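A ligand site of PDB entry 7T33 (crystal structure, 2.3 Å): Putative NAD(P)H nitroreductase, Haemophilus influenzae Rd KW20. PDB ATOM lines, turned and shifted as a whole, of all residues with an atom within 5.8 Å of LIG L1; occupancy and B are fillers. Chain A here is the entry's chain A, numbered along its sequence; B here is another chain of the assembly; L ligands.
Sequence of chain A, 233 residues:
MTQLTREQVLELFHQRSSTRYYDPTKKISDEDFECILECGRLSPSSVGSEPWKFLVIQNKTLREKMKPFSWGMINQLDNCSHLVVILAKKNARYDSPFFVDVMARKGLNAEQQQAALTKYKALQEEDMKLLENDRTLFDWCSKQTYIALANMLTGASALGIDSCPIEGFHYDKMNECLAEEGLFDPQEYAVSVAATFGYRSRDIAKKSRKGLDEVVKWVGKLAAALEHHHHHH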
ATOM      1  N   ARG A  16      -4.246 -32.532  15.854  1.00  0.00           N
ATOM      2  CA  ARG A  16      -4.223 -31.180  15.233  1.00  0.00           C
ATOM      3  C   ARG A  16      -5.043 -30.245  16.106  1.00  0.00           C
ATOM      4  O   ARG A  16      -6.101 -30.647  16.481  1.00  0.00           O
ATOM      5  CB  ARG A  16      -4.789 -31.192  13.826  1.00  0.00           C
ATOM      6  CG  ARG A  16      -4.729 -29.855  13.114  1.00  0.00           C
ATOM      7  CD  ARG A  16      -6.049 -29.337  12.626  1.00  0.00           C
ATOM      8  NE  ARG A  16      -7.168 -29.749  13.433  1.00  0.00           N
ATOM      9  CZ  ARG A  16      -7.808 -28.987  14.277  1.00  0.00           C
ATOM     10  NH1 ARG A  16      -7.448 -27.731  14.444  1.00  0.00           N
ATOM     11  NH2 ARG A  16      -8.804 -29.465  14.972  1.00  0.00           N
ATOM     12  N   SER A  17      -4.538 -29.075  16.453  1.00  0.00           N
ATOM     13  CA  SER A  17      -5.316 -28.140  17.311  1.00  0.00           C
ATOM     14  C   SER A  17      -5.135 -26.721  16.814  1.00  0.00           C
ATOM     15  O   SER A  17      -4.142 -26.475  16.187  1.00  0.00           O
ATOM     16  CB  SER A  17      -4.878 -28.243  18.710  1.00  0.00           C
ATOM     17  OG  SER A  17      -5.586 -29.265  19.365  1.00  0.00           O
ATOM     18  N   SER A  18      -6.067 -25.837  17.131  1.00  0.00           N
ATOM     19  CA  SER A  18      -5.977 -24.419  16.728  1.00  0.00           C
ATOM     20  C   SER A  18      -4.957 -23.704  17.606  1.00  0.00           C
ATOM     21  O   SER A  18      -5.187 -23.560  18.759  1.00  0.00           O
ATOM     22  CB  SER A  18      -7.309 -23.784  16.772  1.00  0.00           C
ATOM     23  OG  SER A  18      -8.110 -24.293  15.722  1.00  0.00           O
ATOM     24  N   ARG A  20      -3.244 -20.493  18.779  1.00  0.00           N
ATOM     25  CA  ARG A  20      -3.424 -19.040  18.881  1.00  0.00           C
ATOM     26  C   ARG A  20      -2.171 -18.289  19.364  1.00  0.00           C
ATOM     27  O   ARG A  20      -2.209 -17.051  19.437  1.00  0.00           O
ATOM     28  CB  ARG A  20      -4.599 -18.729  19.811  1.00  0.00           C
ATOM     29  CG  ARG A  20      -5.935 -18.778  19.124  1.00  0.00           C
ATOM     30  CD  ARG A  20      -6.994 -19.438  19.986  1.00  0.00           C
ATOM     31  NE  ARG A  20      -7.848 -20.347  19.225  1.00  0.00           N
ATOM     32  CZ  ARG A  20      -8.732 -21.186  19.780  1.00  0.00           C
ATOM     33  NH1 ARG A  20      -8.886 -21.245  21.102  1.00  0.00           N
ATOM     34  NH2 ARG A  20      -9.466 -21.977  19.006  1.00  0.00           N
ATOM     35  N   GLY A  72      -9.306 -11.944  14.851  1.00  0.00           N
ATOM     36  CA  GLY A  72      -9.076 -13.392  15.013  1.00  0.00           C
ATOM     37  C   GLY A  72      -7.613 -13.816  14.976  1.00  0.00           C
ATOM     38  O   GLY A  72      -7.338 -14.878  15.467  1.00  0.00           O
ATOM     39  N   MET A  73      -6.722 -13.036  14.381  1.00  0.00           N
ATOM     40  CA  MET A  73      -5.308 -13.449  14.313  1.00  0.00           C
ATOM     41  C   MET A  73      -4.383 -12.279  14.664  1.00  0.00           C
ATOM     42  O   MET A  73      -3.202 -12.381  14.402  1.00  0.00           O
ATOM     43  CB  MET A  73      -4.987 -13.953  12.919  1.00  0.00           C
ATOM     44  CG  MET A  73      -5.437 -13.060  11.854  1.00  0.00           C
ATOM     45  SD  MET A  73      -4.822 -13.636  10.327  1.00  0.00           S
ATOM     46  CE  MET A  73      -5.686 -12.570   9.199  1.00  0.00           C
ATOM     47  N   GLN A  76      -1.339 -13.390  16.302  1.00  0.00           N
ATOM     48  CA  GLN A  76      -0.802 -14.563  15.592  1.00  0.00           C
ATOM     49  C   GLN A  76      -0.016 -14.040  14.396  1.00  0.00           C
ATOM     50  O   GLN A  76       0.947 -14.663  14.000  1.00  0.00           O
ATOM     51  CB  GLN A  76      -2.038 -15.361  15.174  1.00  0.00           C
ATOM     52  CG  GLN A  76      -1.798 -16.716  14.539  1.00  0.00           C
ATOM     53  CD  GLN A  76      -3.120 -17.428  14.350  1.00  0.00           C
ATOM     54  OE1 GLN A  76      -4.166 -16.972  14.775  1.00  0.00           O
ATOM     55  NE2 GLN A  76      -3.047 -18.588  13.720  1.00  0.00           N
ATOM     56  N   TYR A 146     -12.624 -24.679   1.265  1.00  0.00           N
ATOM     57  CA  TYR A 146     -12.551 -25.238   2.606  1.00  0.00           C
ATOM     58  C   TYR A 146     -12.047 -26.673   2.600  1.00  0.00           C
ATOM     59  O   TYR A 146     -11.572 -27.154   3.624  1.00  0.00           O
ATOM     60  CB  TYR A 146     -13.916 -25.179   3.321  1.00  0.00           C
ATOM     61  CG  TYR A 146     -14.167 -23.840   3.944  1.00  0.00           C
ATOM     62  CD1 TYR A 146     -14.126 -22.675   3.182  1.00  0.00           C
ATOM     63  CD2 TYR A 146     -14.422 -23.720   5.317  1.00  0.00           C
ATOM     64  CE1 TYR A 146     -14.351 -21.411   3.754  1.00  0.00           C
ATOM     65  CE2 TYR A 146     -14.641 -22.473   5.905  1.00  0.00           C
ATOM     66  CZ  TYR A 146     -14.597 -21.323   5.117  1.00  0.00           C
ATOM     67  OH  TYR A 146     -14.821 -20.090   5.686  1.00  0.00           O
ATOM     68  N   LEU A 149      -8.307 -26.036   2.508  1.00  0.00           N
ATOM     69  CA  LEU A 149      -7.927 -25.575   3.833  1.00  0.00           C
ATOM     70  C   LEU A 149      -7.778 -26.745   4.796  1.00  0.00           C
ATOM     71  O   LEU A 149      -6.738 -26.905   5.462  1.00  0.00           O
ATOM     72  CB  LEU A 149      -8.974 -24.586   4.355  1.00  0.00           C
ATOM     73  CG  LEU A 149      -8.950 -24.359   5.873  1.00  0.00           C
ATOM     74  CD1 LEU A 149      -7.753 -23.482   6.264  1.00  0.00           C
ATOM     75  CD2 LEU A 149     -10.273 -23.789   6.408  1.00  0.00           C
ATOM     76  N   CYS A 164      -3.698 -22.732  12.589  1.00  0.00           N
ATOM     77  CA  CYS A 164      -4.979 -22.200  13.009  1.00  0.00           C
ATOM     78  C   CYS A 164      -5.740 -21.715  11.764  1.00  0.00           C
ATOM     79  O   CYS A 164      -5.180 -20.949  10.973  1.00  0.00           O
ATOM     80  CB  CYS A 164      -4.818 -21.066  14.016  1.00  0.00           C
ATOM     81  SG  CYS A 164      -6.379 -20.614  14.838  1.00  0.00           S
ATOM     82  N   PRO A 165      -6.957 -22.198  11.493  1.00  0.00           N
ATOM     83  CA  PRO A 165      -7.760 -21.665  10.419  1.00  0.00           C
ATOM     84  C   PRO A 165      -8.352 -20.345  10.904  1.00  0.00           C
ATOM     85  O   PRO A 165      -8.606 -20.226  12.018  1.00  0.00           O
ATOM     86  CB  PRO A 165      -8.846 -22.707  10.234  1.00  0.00           C
ATOM     87  CG  PRO A 165      -8.960 -23.333  11.573  1.00  0.00           C
ATOM     88  CD  PRO A 165      -7.554 -23.354  12.099  1.00  0.00           C
ATOM     89  N   ILE A 166      -8.561 -19.382  10.013  1.00  0.00           N
ATOM     90  CA  ILE A 166      -9.015 -18.038  10.464  1.00  0.00           C
ATOM     91  C   ILE A 166     -10.180 -17.510   9.629  1.00  0.00           C
ATOM     92  O   ILE A 166     -10.068 -17.429   8.447  1.00  0.00           O
ATOM     93  CB  ILE A 166      -7.844 -17.037  10.369  1.00  0.00           C
ATOM     94  CG1 ILE A 166      -6.596 -17.456  11.141  1.00  0.00           C
ATOM     95  CG2 ILE A 166      -8.285 -15.649  10.741  1.00  0.00           C
ATOM     96  CD1 ILE A 166      -6.817 -17.619  12.597  1.00  0.00           C
ATOM     97  N   GLU A 167     -11.242 -17.105  10.292  1.00  0.00           N
ATOM     98  CA  GLU A 167     -12.356 -16.385   9.633  1.00  0.00           C
ATOM     99  C   GLU A 167     -12.541 -15.052  10.357  1.00  0.00           C
ATOM    100  O   GLU A 167     -13.319 -14.257   9.920  1.00  0.00           O
ATOM    101  CB  GLU A 167     -13.669 -17.138   9.816  1.00  0.00           C
ATOM    102  CG  GLU A 167     -13.941 -18.174   8.773  1.00  0.00           C
ATOM    103  CD  GLU A 167     -15.249 -18.917   8.948  1.00  0.00           C
ATOM    104  OE1 GLU A 167     -15.926 -18.649   9.867  1.00  0.00           O
ATOM    105  OE2 GLU A 167     -15.528 -19.753   8.164  1.00  0.00           O
ATOM    106  N   GLY A 168     -11.795 -14.830  11.434  1.00  0.00           N
ATOM    107  CA  GLY A 168     -11.972 -13.653  12.285  1.00  0.00           C
ATOM    108  C   GLY A 168     -11.370 -12.402  11.735  1.00  0.00           C
ATOM    109  O   GLY A 168     -10.400 -11.960  12.265  1.00  0.00           O
ATOM    110  N   PHE A 169     -11.972 -11.866  10.695  1.00  0.00           N
ATOM    111  CA  PHE A 169     -11.542 -10.592  10.084  1.00  0.00           C
ATOM    112  C   PHE A 169     -12.713 -10.004   9.304  1.00  0.00           C
ATOM    113  O   PHE A 169     -13.654 -10.696   9.060  1.00  0.00           O
ATOM    114  CB  PHE A 169     -10.253 -10.764   9.274  1.00  0.00           C
ATOM    115  CG  PHE A 169     -10.317 -11.769   8.167  1.00  0.00           C
ATOM    116  CD1 PHE A 169      -9.708 -13.002   8.305  1.00  0.00           C
ATOM    117  CD2 PHE A 169     -10.976 -11.495   6.992  1.00  0.00           C
ATOM    118  CE1 PHE A 169      -9.776 -13.950   7.296  1.00  0.00           C
ATOM    119  CE2 PHE A 169     -11.026 -12.427   5.987  1.00  0.00           C
ATOM    120  CZ  PHE A 169     -10.420 -13.648   6.138  1.00  0.00           C
ATOM    121  N   VAL A 193     -11.213 -17.683   3.118  1.00  0.00           N
ATOM    122  CA  VAL A 193     -10.774 -18.075   4.486  1.00  0.00           C
ATOM    123  C   VAL A 193      -9.251 -17.923   4.567  1.00  0.00           C
ATOM    124  O   VAL A 193      -8.626 -17.854   3.541  1.00  0.00           O
ATOM    125  CB  VAL A 193     -11.235 -19.497   4.835  1.00  0.00           C
ATOM    126  CG1 VAL A 193     -10.434 -20.558   4.133  1.00  0.00           C
ATOM    127  CG2 VAL A 193     -11.277 -19.760   6.320  1.00  0.00           C
ATOM    128  N   LYS A 207      -9.049 -31.289  23.796  1.00  0.00           N
ATOM    129  CA  LYS A 207      -9.867 -31.420  22.568  1.00  0.00           C
ATOM    130  C   LYS A 207     -11.330 -31.479  23.002  1.00  0.00           C
ATOM    131  O   LYS A 207     -11.630 -32.297  23.837  1.00  0.00           O
ATOM    132  CB  LYS A 207      -9.460 -32.721  21.888  1.00  0.00           C
ATOM    133  CG  LYS A 207     -10.062 -32.959  20.519  1.00  0.00           C
ATOM    134  CD  LYS A 207      -9.789 -31.841  19.570  1.00  0.00           C
ATOM    135  CE  LYS A 207      -8.335 -31.686  19.220  1.00  0.00           C
ATOM    136  NZ  LYS A 207      -8.187 -30.930  17.967  1.00  0.00           N
ATOM    137  N   SER A 208     -12.201 -30.633  22.471  1.00  0.00           N
ATOM    138  CA  SER A 208     -13.610 -30.676  22.903  1.00  0.00           C
ATOM    139  C   SER A 208     -14.533 -30.773  21.691  1.00  0.00           C
ATOM    140  O   SER A 208     -14.535 -29.849  20.891  1.00  0.00           O
ATOM    141  CB  SER A 208     -13.950 -29.483  23.701  1.00  0.00           C
ATOM    142  OG  SER A 208     -15.343 -29.319  23.761  1.00  0.00           O
ATOM    143  N   ARG A 209     -15.290 -31.841  21.587  1.00  0.00           N
ATOM    144  CA  ARG A 209     -16.234 -32.023  20.469  1.00  0.00           C
ATOM    145  C   ARG A 209     -17.492 -32.726  20.981  1.00  0.00           C
ATOM    146  O   ARG A 209     -17.423 -33.381  22.008  1.00  0.00           O
ATOM    147  CB  ARG A 209     -15.657 -32.964  19.426  1.00  0.00           C
ATOM    148  CG  ARG A 209     -14.512 -32.383  18.634  1.00  0.00           C
ATOM    149  CD  ARG A 209     -14.999 -31.241  17.793  1.00  0.00           C
ATOM    150  NE  ARG A 209     -13.886 -30.883  16.988  1.00  0.00           N
ATOM    151  CZ  ARG A 209     -12.869 -30.190  17.425  1.00  0.00           C
ATOM    152  NH1 ARG A 209     -12.835 -29.793  18.671  1.00  0.00           N
ATOM    153  NH2 ARG A 209     -11.874 -29.908  16.627  1.00  0.00           N
ATOM    154  N   LEU B  42     -13.906 -34.848  14.591  1.00  0.00           N
ATOM    155  CA  LEU B  42     -12.788 -34.120  15.179  1.00  0.00           C
ATOM    156  C   LEU B  42     -12.361 -32.927  14.339  1.00  0.00           C
ATOM    157  O   LEU B  42     -11.433 -32.216  14.724  1.00  0.00           O
ATOM    158  CB  LEU B  42     -11.601 -35.077  15.362  1.00  0.00           C
ATOM    159  CG  LEU B  42     -11.797 -36.321  16.245  1.00  0.00           C
ATOM    160  CD1 LEU B  42     -10.635 -37.281  16.076  1.00  0.00           C
ATOM    161  CD2 LEU B  42     -11.965 -35.951  17.697  1.00  0.00           C
ATOM    162  N   SER B  43     -13.022 -32.688  13.213  1.00  0.00           N
ATOM    163  CA  SER B  43     -12.592 -31.619  12.322  1.00  0.00           C
ATOM    164  C   SER B  43     -12.742 -30.260  13.013  1.00  0.00           C
ATOM    165  O   SER B  43     -13.613 -30.072  13.868  1.00  0.00           O
ATOM    166  CB  SER B  43     -13.407 -31.644  11.026  1.00  0.00           C
ATOM    167  OG  SER B  43     -13.106 -32.820  10.274  1.00  0.00           O
ATOM    168  N   PRO B  44     -11.898 -29.291  12.681  1.00  0.00           N
ATOM    169  CA  PRO B  44     -12.096 -27.953  13.203  1.00  0.00           C
ATOM    170  C   PRO B  44     -13.347 -27.360  12.595  1.00  0.00           C
ATOM    171  O   PRO B  44     -13.860 -27.840  11.581  1.00  0.00           O
ATOM    172  CB  PRO B  44     -10.835 -27.194  12.768  1.00  0.00           C
ATOM    173  CG  PRO B  44     -10.354 -27.936  11.563  1.00  0.00           C
ATOM    174  CD  PRO B  44     -10.688 -29.376  11.835  1.00  0.00           C
ATOM    175  N   SER B  45     -13.869 -26.330  13.250  1.00  0.00           N
ATOM    176  CA  SER B  45     -15.027 -25.611  12.727  1.00  0.00           C
ATOM    177  C   SER B  45     -15.007 -24.201  13.294  1.00  0.00           C
ATOM    178  O   SER B  45     -14.521 -23.966  14.406  1.00  0.00           O
ATOM    179  CB  SER B  45     -16.350 -26.296  13.086  1.00  0.00           C
ATOM    180  OG  SER B  45     -16.512 -26.366  14.483  1.00  0.00           O
ATOM    181  N   SER B  46     -15.513 -23.269  12.496  1.00  0.00           N
ATOM    182  CA  SER B  46     -15.597 -21.881  12.923  1.00  0.00           C
ATOM    183  C   SER B  46     -16.286 -21.767  14.278  1.00  0.00           C
ATOM    184  O   SER B  46     -17.358 -22.330  14.471  1.00  0.00           O
ATOM    185  CB  SER B  46     -16.371 -21.057  11.894  1.00  0.00           C
ATOM    186  OG  SER B  46     -16.421 -19.712  12.321  1.00  0.00           O
ATOM    187  N   VAL B  47     -15.658 -21.018  15.181  1.00  0.00           N
ATOM    188  CA  VAL B  47     -16.072 -20.803  16.581  1.00  0.00           C
ATOM    189  C   VAL B  47     -16.533 -22.087  17.258  1.00  0.00           C
ATOM    190  O   VAL B  47     -17.429 -22.065  18.112  1.00  0.00           O
ATOM    191  CB  VAL B  47     -17.155 -19.691  16.702  1.00  0.00           C
ATOM    192  CG1 VAL B  47     -16.648 -18.358  16.182  1.00  0.00           C
ATOM    193  CG2 VAL B  47     -18.474 -20.054  15.996  1.00  0.00           C
ATOM    194  N   GLY B  48     -15.975 -23.223  16.857  1.00  0.00           N
ATOM    195  CA  GLY B  48     -16.319 -24.519  17.435  1.00  0.00           C
ATOM    196  C   GLY B  48     -17.772 -24.858  17.249  1.00  0.00           C
ATOM    197  O   GLY B  48     -18.313 -25.565  18.037  1.00  0.00           O
ATOM    198  N   LYS B 106     -18.574 -25.022  26.314  1.00  0.00           N
ATOM    199  CA  LYS B 106     -17.281 -24.340  26.623  1.00  0.00           C
ATOM    200  C   LYS B 106     -17.353 -23.799  28.046  1.00  0.00           C
ATOM    201  O   LYS B 106     -16.388 -23.265  28.567  1.00  0.00           O
ATOM    202  CB  LYS B 106     -16.978 -23.231  25.632  1.00  0.00           C
ATOM    203  CG  LYS B 106     -16.351 -23.703  24.331  1.00  0.00           C
ATOM    204  CD  LYS B 106     -16.503 -22.729  23.208  1.00  0.00           C
ATOM    205  CE  LYS B 106     -16.839 -23.417  21.899  1.00  0.00           C
ATOM    206  NZ  LYS B 106     -15.944 -22.971  20.808  1.00  0.00           N
ATOM    207  N   GLN B 144     -18.155 -25.215   6.793  1.00  0.00           N
ATOM    208  CA  GLN B 144     -17.566 -26.001   7.875  1.00  0.00           C
ATOM    209  C   GLN B 144     -17.665 -27.498   7.567  1.00  0.00           C
ATOM    210  O   GLN B 144     -16.679 -28.228   7.698  1.00  0.00           O
ATOM    211  CB  GLN B 144     -18.252 -25.697   9.226  1.00  0.00           C
ATOM    212  CG  GLN B 144     -18.441 -24.213   9.595  1.00  0.00           C
ATOM    213  CD  GLN B 144     -17.231 -23.329   9.303  1.00  0.00           C
ATOM    214  OE1 GLN B 144     -16.112 -23.598   9.744  1.00  0.00           O
ATOM    215  NE2 GLN B 144     -17.461 -22.243   8.557  1.00  0.00           N
ATOM    216  N   ILE B 147     -15.049 -29.100   5.490  1.00  0.00           N
ATOM    217  CA  ILE B 147     -13.833 -29.473   6.212  1.00  0.00           C
ATOM    218  C   ILE B 147     -13.951 -30.907   6.697  1.00  0.00           C
ATOM    219  O   ILE B 147     -13.026 -31.714   6.533  1.00  0.00           O
ATOM    220  CB  ILE B 147     -13.582 -28.515   7.391  1.00  0.00           C
ATOM    221  CG1 ILE B 147     -13.335 -27.094   6.915  1.00  0.00           C
ATOM    222  CG2 ILE B 147     -12.425 -29.040   8.261  1.00  0.00           C
ATOM    223  CD1 ILE B 147     -13.020 -26.178   8.108  1.00  0.00           C
HETATM  224  N1  LIG L   1      -9.790 -19.611  15.629  1.00  0.00           N
HETATM  225  C1  LIG L   1      -9.339 -18.395  15.903  1.00  0.00           C
HETATM  226  O1  LIG L   1      -8.676 -18.235  16.883  1.00  0.00           O
HETATM  227  N2  LIG L   1      -9.581 -17.352  15.113  1.00  0.00           N
HETATM  228  C2  LIG L   1     -10.282 -17.530  14.028  1.00  0.00           C
HETATM  229  O2  LIG L   1     -10.447 -16.545  13.384  1.00  0.00           O
HETATM  230  C3  LIG L   1     -10.775 -18.787  13.711  1.00  0.00           C
HETATM  231  N3  LIG L   1     -11.481 -19.016  12.642  1.00  0.00           N
HETATM  232  C4  LIG L   1     -11.709 -20.239  12.246  1.00  0.00           C
HETATM  233  C5  LIG L   1     -12.237 -20.452  11.016  1.00  0.00           C
HETATM  234  C6  LIG L   1     -12.517 -21.722  10.621  1.00  0.00           C
HETATM  235  C7  LIG L   1     -13.041 -21.926   9.382  1.00  0.00           C
HETATM  236  C8  LIG L   1     -12.271 -22.770  11.440  1.00  0.00           C
HETATM  237  C9  LIG L   1     -12.537 -24.019  11.020  1.00  0.00           C
HETATM  238  C10 LIG L   1     -11.746 -22.547  12.669  1.00  0.00           C
HETATM  239  C11 LIG L   1     -11.467 -21.295  13.088  1.00  0.00           C
HETATM  240  N4  LIG L   1     -10.945 -21.067  14.287  1.00  0.00           N
HETATM  241  C12 LIG L   1     -10.522 -19.829  14.551  1.00  0.00           C
HETATM  242  C13 LIG L   1     -10.615 -22.156  15.221  1.00  0.00           C
HETATM  243  C14 LIG L   1     -11.757 -22.872  15.892  1.00  0.00           C
HETATM  244  O3  LIG L   1     -12.229 -22.026  16.872  1.00  0.00           O
HETATM  245  C15 LIG L   1     -11.255 -24.202  16.399  1.00  0.00           C
HETATM  246  O4  LIG L   1     -11.019 -24.919  15.284  1.00  0.00           O
HETATM  247  C16 LIG L   1     -12.294 -25.046  17.070  1.00  0.00           C
HETATM  248  O5  LIG L   1     -12.828 -24.350  18.153  1.00  0.00           O
HETATM  249  C17 LIG L   1     -11.777 -26.408  17.546  1.00  0.00           C
HETATM  250  O6  LIG L   1     -10.597 -26.409  18.220  1.00  0.00           O
HETATM  251  P1  LIG L   1      -9.542 -27.112  17.751  1.00  0.00           P
HETATM  252  O7  LIG L   1      -9.889 -28.406  18.027  1.00  0.00           O
HETATM  253  O8  LIG L   1      -9.428 -26.864  16.426  1.00  0.00           O
HETATM  254  O9  LIG L   1      -8.482 -26.596  18.440  1.00  0.00           O
HETATM  255  N1  LG2 L   2     -12.408 -15.422  16.677  1.00  0.00           N
HETATM  256  C1  LG2 L   2     -12.387 -16.756  17.137  1.00  0.00           C
HETATM  257  C2  LG2 L   2     -12.889 -17.768  16.334  1.00  0.00           C
HETATM  258  C3  LG2 L   2     -13.453 -17.476  15.099  1.00  0.00           C
HETATM  259  C4  LG2 L   2     -13.492 -16.157  14.648  1.00  0.00           C
HETATM  260  C5  LG2 L   2     -12.966 -15.132  15.420  1.00  0.00           C
HETATM  261  C6  LG2 L   2     -12.887 -19.089  16.778  1.00  0.00           C
HETATM  262  O1  LG2 L   2     -13.156 -19.993  15.956  1.00  0.00           O
HETATM  263  O2  LG2 L   2     -12.469 -19.375  17.935  1.00  0.00           O
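The backbone carbonyl oxygen of Pro 165 lies close to a nitrogen (N3) of LIG L1, 3.2 Å away.
Residues that only touch LIG L1: Ser 17 (3.7 Å), Tyr 146 (3.9 Å), Ile 166 (3.4 Å), Pro 44 of chain B (3.4 Å), Ser 45 of chain B (3.3 Å), Ser 46 of chain B (3.4 Å), Val 47 of chain B (3.95 Å), Gly 48 of chain B (3.6 Å), Gln 144 of chain B (3.5 Å) and Ile 147 of chain B (3.7 Å).
Hydrophobic or aromatic side chains within 4 Å of LIG L1: Tyr 146, Pro 165, Ile 166, Pro 44 of chain B and Ile 147 of chain B.
Of the 29 residues printed, 20 come within 4 Å of LIG L1.
The nearest printed residue that does not touch LIG L1 is Val 193 (4.1 Å).
The backbone NH (N) of Ser 18 is in hydrogen-bond range of an oxygen (O9) of LIG L1.
The side-chain hydroxyl (OG) of Ser 18 sits at hydrogen-bond distance from an oxygen (O8) of LIG L1, 3.0 Å away.
O7 of LIG L1 is in salt-bridge range of NH2 of Arg 209, at 2.9 Å.
An oxygen (O2) of LIG L1 is in hydrogen-bond range of the backbone NH of Gly 168, 2.9 Å away.
An oxygen (O8) of LIG L1 lies within salt-bridge range of the guanidinium group (NH1) of Arg 16, at 2.9 Å.
The backbone NH of Glu 167 is in hydrogen-bond range of a nitrogen (N3) of LIG L1, 3.0 Å away.
The side-chain amino group of Lys 207 lies within salt-bridge range of an oxygen (O7) of LIG L1 (3.0 Å).
The guanidinium group of Arg 20 lies within hydrogen-bond range of an oxygen (O1) of LIG L1 (3.3 Å).
N2 of LIG L1 lies within hydrogen-bond range of O of Gly 72.
The side-chain sulfur of Cys 164 sits at hydrogen-bond distance from a nitrogen (N1) of LIG L1 (3.6 Å).
The backbone NH of Val 47 of chain B sits at hydrogen-bond distance from an oxygen (O1) of LG2 L2 (2.8 Å).
The guanidinium group (NE) of Arg 209 is in hydrogen-bond range of the backbone carbonyl oxygen (O) of Ser 43 of chain B, at 3.2 Å.
The backbone carbonyl oxygen of Gly 168 sits at hydrogen-bond distance from the backbone NH of Gly 72 (2.8 Å).
The backbone carbonyl oxygen (O) of Arg 16 lies within hydrogen-bond range of the side-chain amino group (NZ) of Lys 207 (2.6 Å).
The side-chain carboxylate (OE1) of Glu 167 sits at hydrogen-bond distance from the side-chain hydroxyl (OG) of Ser 46 of chain B, 2.7 Å away.
The side-chain carboxylate (OE2) of Glu 167 lies within hydrogen-bond range of the side-chain amide nitrogen (NE2) of Gln 144 of chain B (3.2 Å).
The side-chain carboxylate of Glu 167 lies within hydrogen-bond range of the side-chain hydroxyl of Tyr 146, at 2.6 Å.
NZ of Lys 207 is in hydrogen-bond range of OG of Ser 17 (3.4 Å).
The backbone NH of Ser 46 of chain B sits at hydrogen-bond distance from the side-chain amide oxygen of Gln 144 of chain B.
O3 of LIG L1 is in hydrogen-bond range of O1 of LG2 L2 (2.4 Å).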
